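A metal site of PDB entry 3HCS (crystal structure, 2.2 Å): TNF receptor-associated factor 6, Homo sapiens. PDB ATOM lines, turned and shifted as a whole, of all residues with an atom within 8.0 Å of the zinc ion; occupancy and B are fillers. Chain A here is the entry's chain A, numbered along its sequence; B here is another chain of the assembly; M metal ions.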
ATOM      1  N   THR A  34      16.193   1.894 -13.357  1.00  0.00           N
ATOM      2  CA  THR A  34      16.876   0.820 -14.082  1.00  0.00           C
ATOM      3  C   THR A  34      15.957   0.223 -15.140  1.00  0.00           C
ATOM      4  O   THR A  34      14.763   0.514 -15.175  1.00  0.00           O
ATOM      5  CB  THR A  34      17.298  -0.311 -13.148  1.00  0.00           C
ATOM      6  OG1 THR A  34      16.125  -0.933 -12.614  1.00  0.00           O
ATOM      7  CG2 THR A  34      18.164   0.225 -12.021  1.00  0.00           C
ATOM      8  N   PRO A  35      16.512  -0.598 -16.046  1.00  0.00           N
ATOM      9  CA  PRO A  35      15.666  -1.201 -17.087  1.00  0.00           C
ATOM     10  C   PRO A  35      14.668  -2.175 -16.482  1.00  0.00           C
ATOM     11  O   PRO A  35      13.607  -2.425 -17.048  1.00  0.00           O
ATOM     12  CB  PRO A  35      16.681  -1.891 -18.005  1.00  0.00           C
ATOM     13  CG  PRO A  35      17.919  -1.026 -17.836  1.00  0.00           C
ATOM     14  CD  PRO A  35      17.944  -0.774 -16.346  1.00  0.00           C
ATOM     15  N   CYS A  36      15.025  -2.708 -15.314  1.00  0.00           N
ATOM     16  CA  CYS A  36      14.177  -3.659 -14.604  1.00  0.00           C
ATOM     17  C   CYS A  36      13.170  -2.966 -13.680  1.00  0.00           C
ATOM     18  O   CYS A  36      12.636  -3.573 -12.759  1.00  0.00           O
ATOM     19  CB  CYS A  36      15.062  -4.615 -13.813  1.00  0.00           C
ATOM     20  SG  CYS A  36      16.375  -3.760 -12.909  1.00  0.00           S
ATOM     21  N   GLY A  37      12.939  -1.673 -13.929  1.00  0.00           N
ATOM     22  CA  GLY A  37      11.960  -0.920 -13.170  1.00  0.00           C
ATOM     23  C   GLY A  37      12.181  -0.598 -11.691  1.00  0.00           C
ATOM     24  O   GLY A  37      11.206  -0.514 -10.946  1.00  0.00           O
ATOM     25  N   HIS A  38      13.429  -0.390 -11.288  1.00  0.00           N
ATOM     26  CA  HIS A  38      13.712  -0.063  -9.892  1.00  0.00           C
ATOM     27  C   HIS A  38      14.391   1.296  -9.759  1.00  0.00           C
ATOM     28  O   HIS A  38      15.307   1.622 -10.510  1.00  0.00           O
ATOM     29  CB  HIS A  38      14.569  -1.153  -9.253  1.00  0.00           C
ATOM     30  CG  HIS A  38      13.846  -2.448  -9.080  1.00  0.00           C
ATOM     31  ND1 HIS A  38      13.766  -3.395 -10.082  1.00  0.00           N
ATOM     32  CD2 HIS A  38      13.120  -2.933  -8.043  1.00  0.00           C
ATOM     33  CE1 HIS A  38      13.025  -4.409  -9.669  1.00  0.00           C
ATOM     34  NE2 HIS A  38      12.618  -4.146  -8.446  1.00  0.00           N
ATOM     35  N   ARG A  39      13.928   2.084  -8.797  1.00  0.00           N
ATOM     36  CA  ARG A  39      14.464   3.420  -8.563  1.00  0.00           C
ATOM     37  C   ARG A  39      15.530   3.453  -7.490  1.00  0.00           C
ATOM     38  O   ARG A  39      15.441   2.749  -6.491  1.00  0.00           O
ATOM     39  CB  ARG A  39      13.341   4.354  -8.148  1.00  0.00           C
ATOM     40  CG  ARG A  39      12.241   4.524  -9.157  1.00  0.00           C
ATOM     41  CD  ARG A  39      11.044   5.059  -8.416  1.00  0.00           C
ATOM     42  NE  ARG A  39      10.118   5.787  -9.273  1.00  0.00           N
ATOM     43  CZ  ARG A  39       9.019   6.369  -8.811  1.00  0.00           C
ATOM     44  NH1 ARG A  39       8.729   6.281  -7.518  1.00  0.00           N
ATOM     45  NH2 ARG A  39       8.225   7.032  -9.638  1.00  0.00           N
ATOM     46  N   PHE A  40      16.538   4.297  -7.694  1.00  0.00           N
ATOM     47  CA  PHE A  40      17.631   4.458  -6.740  1.00  0.00           C
ATOM     48  C   PHE A  40      18.180   5.880  -6.820  1.00  0.00           C
ATOM     49  O   PHE A  40      17.922   6.615  -7.788  1.00  0.00           O
ATOM     50  CB  PHE A  40      18.794   3.517  -7.057  1.00  0.00           C
ATOM     51  CG  PHE A  40      18.431   2.057  -7.126  1.00  0.00           C
ATOM     52  CD1 PHE A  40      18.069   1.478  -8.338  1.00  0.00           C
ATOM     53  CD2 PHE A  40      18.526   1.255  -5.984  1.00  0.00           C
ATOM     54  CE1 PHE A  40      17.807   0.115  -8.420  1.00  0.00           C
ATOM     55  CE2 PHE A  40      18.265  -0.118  -6.064  1.00  0.00           C
ATOM     56  CZ  PHE A  40      17.901  -0.688  -7.278  1.00  0.00           C
ATOM     57  N   ILE A  45      23.128   3.711  -6.532  1.00  0.00           N
ATOM     58  CA  ILE A  45      23.169   2.664  -7.539  1.00  0.00           C
ATOM     59  C   ILE A  45      24.522   2.600  -8.235  1.00  0.00           C
ATOM     60  O   ILE A  45      25.035   1.517  -8.517  1.00  0.00           O
ATOM     61  CB  ILE A  45      22.039   2.837  -8.594  1.00  0.00           C
ATOM     62  CG1 ILE A  45      22.049   1.668  -9.572  1.00  0.00           C
ATOM     63  CG2 ILE A  45      22.189   4.161  -9.321  1.00  0.00           C
ATOM     64  CD1 ILE A  45      21.726   0.332  -8.933  1.00  0.00           C
ATOM     65  N   LYS A  55      24.857  -5.190 -11.626  1.00  0.00           N
ATOM     66  CA  LYS A  55      23.530  -5.772 -11.512  1.00  0.00           C
ATOM     67  C   LYS A  55      22.683  -4.950 -10.558  1.00  0.00           C
ATOM     68  O   LYS A  55      23.198  -4.184  -9.748  1.00  0.00           O
ATOM     69  CB  LYS A  55      23.624  -7.197 -10.996  1.00  0.00           C
ATOM     70  CG  LYS A  55      24.256  -7.319  -9.623  1.00  0.00           C
ATOM     71  CD  LYS A  55      24.293  -8.754  -9.149  1.00  0.00           C
ATOM     72  CE  LYS A  55      24.831  -8.856  -7.732  1.00  0.00           C
ATOM     73  NZ  LYS A  55      24.879 -10.262  -7.236  1.00  0.00           N
ATOM     74  N   CYS A  56      21.372  -5.104 -10.675  1.00  0.00           N
ATOM     75  CA  CYS A  56      20.440  -4.408  -9.817  1.00  0.00           C
ATOM     76  C   CYS A  56      20.455  -5.153  -8.479  1.00  0.00           C
ATOM     77  O   CYS A  56      20.252  -6.365  -8.436  1.00  0.00           O
ATOM     78  CB  CYS A  56      19.055  -4.451 -10.441  1.00  0.00           C
ATOM     79  SG  CYS A  56      17.783  -3.825  -9.359  1.00  0.00           S
ATOM     80  N   PRO A  57      20.714  -4.433  -7.378  1.00  0.00           N
ATOM     81  CA  PRO A  57      20.761  -5.012  -6.030  1.00  0.00           C
ATOM     82  C   PRO A  57      19.497  -5.772  -5.626  1.00  0.00           C
ATOM     83  O   PRO A  57      19.578  -6.769  -4.913  1.00  0.00           O
ATOM     84  CB  PRO A  57      20.999  -3.798  -5.136  1.00  0.00           C
ATOM     85  CG  PRO A  57      21.792  -2.894  -6.010  1.00  0.00           C
ATOM     86  CD  PRO A  57      21.059  -3.002  -7.322  1.00  0.00           C
ATOM     87  N   VAL A  58      18.346  -5.335  -6.110  1.00  0.00           N
ATOM     88  CA  VAL A  58      17.090  -5.954  -5.733  1.00  0.00           C
ATOM     89  C   VAL A  58      16.726  -7.286  -6.394  1.00  0.00           C
ATOM     90  O   VAL A  58      16.028  -8.114  -5.808  1.00  0.00           O
ATOM     91  CB  VAL A  58      15.901  -4.997  -5.945  1.00  0.00           C
ATOM     92  CG1 VAL A  58      16.229  -3.633  -5.368  1.00  0.00           C
ATOM     93  CG2 VAL A  58      15.583  -4.901  -7.425  1.00  0.00           C
ATOM     94  N   ASP A  59      17.167  -7.496  -7.633  1.00  0.00           N
ATOM     95  CA  ASP A  59      16.824  -8.730  -8.330  1.00  0.00           C
ATOM     96  C   ASP A  59      17.975  -9.350  -9.120  1.00  0.00           C
ATOM     97  O   ASP A  59      17.766 -10.249  -9.931  1.00  0.00           O
ATOM     98  CB  ASP A  59      15.636  -8.474  -9.255  1.00  0.00           C
ATOM     99  CG  ASP A  59      15.876  -7.338 -10.234  1.00  0.00           C
ATOM    100  OD1 ASP A  59      14.881  -6.861 -10.839  1.00  0.00           O
ATOM    101  OD2 ASP A  59      17.041  -6.929 -10.417  1.00  0.00           O
ATOM    102  N   ASN A  60      19.182  -8.845  -8.902  1.00  0.00           N
ATOM    103  CA  ASN A  60      20.376  -9.340  -9.581  1.00  0.00           C
ATOM    104  C   ASN A  60      20.359  -9.261 -11.096  1.00  0.00           C
ATOM    105  O   ASN A  60      21.211  -9.854 -11.750  1.00  0.00           O
ATOM    106  CB  ASN A  60      20.662 -10.783  -9.153  1.00  0.00           C
ATOM    107  CG  ASN A  60      21.092 -10.875  -7.718  1.00  0.00           C
ATOM    108  OD1 ASN A  60      21.964 -10.128  -7.260  1.00  0.00           O
ATOM    109  ND2 ASN A  60      20.492 -11.800  -6.976  1.00  0.00           N
ATOM    110  N   GLU A  61      19.407  -8.534 -11.665  1.00  0.00           N
ATOM    111  CA  GLU A  61      19.369  -8.385 -13.113  1.00  0.00           C
ATOM    112  C   GLU A  61      20.636  -7.652 -13.538  1.00  0.00           C
ATOM    113  O   GLU A  61      21.084  -6.741 -12.846  1.00  0.00           O
ATOM    114  CB  GLU A  61      18.137  -7.572 -13.533  1.00  0.00           C
ATOM    115  CG  GLU A  61      16.811  -8.321 -13.450  1.00  0.00           C
ATOM    116  CD  GLU A  61      16.618  -9.307 -14.589  1.00  0.00           C
ATOM    117  OE1 GLU A  61      16.692  -8.888 -15.762  1.00  0.00           O
ATOM    118  OE2 GLU A  61      16.394 -10.514 -14.312  1.00  0.00           O
ATOM    119  N   ILE A  62      21.216  -8.051 -14.667  1.00  0.00           N
ATOM    120  CA  ILE A  62      22.436  -7.402 -15.171  1.00  0.00           C
ATOM    121  C   ILE A  62      22.143  -5.921 -15.397  1.00  0.00           C
ATOM    122  O   ILE A  62      21.184  -5.562 -16.062  1.00  0.00           O
ATOM    123  CB  ILE A  62      22.910  -8.010 -16.519  1.00  0.00           C
ATOM    124  CG1 ILE A  62      23.342  -9.469 -16.328  1.00  0.00           C
ATOM    125  CG2 ILE A  62      24.069  -7.194 -17.067  1.00  0.00           C
ATOM    126  CD1 ILE A  62      24.681  -9.630 -15.621  1.00  0.00           C
ATOM    127  N   LEU A  63      23.008  -5.067 -14.860  1.00  0.00           N
ATOM    128  CA  LEU A  63      22.838  -3.617 -14.971  1.00  0.00           C
ATOM    129  C   LEU A  63      24.104  -2.856 -15.302  1.00  0.00           C
ATOM    130  O   LEU A  63      25.133  -3.009 -14.653  1.00  0.00           O
ATOM    131  CB  LEU A  63      22.285  -3.072 -13.650  1.00  0.00           C
ATOM    132  CG  LEU A  63      22.234  -1.548 -13.508  1.00  0.00           C
ATOM    133  CD1 LEU A  63      21.180  -0.989 -14.441  1.00  0.00           C
ATOM    134  CD2 LEU A  63      21.927  -1.193 -12.068  1.00  0.00           C
ATOM    135  N   ARG B  76       4.860  -1.489 -13.564  1.00  0.00           N
ATOM    136  CA  ARG B  76       4.684  -2.459 -12.486  1.00  0.00           C
ATOM    137  C   ARG B  76       3.633  -1.988 -11.473  1.00  0.00           C
ATOM    138  O   ARG B  76       2.789  -2.776 -11.026  1.00  0.00           O
ATOM    139  CB  ARG B  76       6.009  -2.713 -11.767  1.00  0.00           C
ATOM    140  CG  ARG B  76       5.882  -3.654 -10.586  1.00  0.00           C
ATOM    141  CD  ARG B  76       7.201  -3.926  -9.884  1.00  0.00           C
ATOM    142  NE  ARG B  76       8.161  -4.571 -10.764  1.00  0.00           N
ATOM    143  CZ  ARG B  76       9.322  -4.030 -11.141  1.00  0.00           C
ATOM    144  NH1 ARG B  76       9.667  -2.817 -10.725  1.00  0.00           N
ATOM    145  NH2 ARG B  76      10.136  -4.697 -11.950  1.00  0.00           N
HETATM  146 ZN    ZN M   1      15.866  -4.338 -10.609  1.00  0.00          ZN
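The side-chain sulfur (SG) of Cys 56 sits close to the side-chain carboxylate (OD2) of Asp 59 (3.4 Å).
SG of Cys 56 lies close to N of Val 58, 3.6 Å away.
The backbone NH of His 38 lies within hydrogen-bond range of the side-chain hydroxyl of Thr 34, 3.1 Å away.
The side-chain carboxylate (OD2) of Asp 59 lies close to the backbone NH (N) of Glu 61 (3.1 Å).
The backbone NH of Cys 56 lies within hydrogen-bond range of the backbone carbonyl oxygen of Glu 61.
The backbone carbonyl oxygen of Cys 36 sits at hydrogen-bond distance from the guanidinium group of Arg 76 of chain B.
N of Cys 36 sits close to OG1 of Thr 34 (3.4 Å).
Thr 34 touches the zinc ion (OG1 to ZN, 3.96 Å).
Val 58 touches the zinc ion (CG2 to ZN, 3.2 Å).
Of the 18 residues printed, 6 come within 4 Å of the zinc ion.
Along chain A the residues within 4 Å of the zinc ion span positions 34 to 59.
The nearest printed residue that does not touch the zinc ion is Glu 61 (4.9 Å).
SG of Cys 56 is bound to the zinc ion, 2.3 Å away.
The zinc ion is bound by a ring nitrogen (ND1) of His 38 (2.4 Å).
The zinc ion is bound by SG of Cys 36 (2.4 Å).
Slightly farther from the zinc ion lies OD1 of Asp 59 (2.7 Å).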
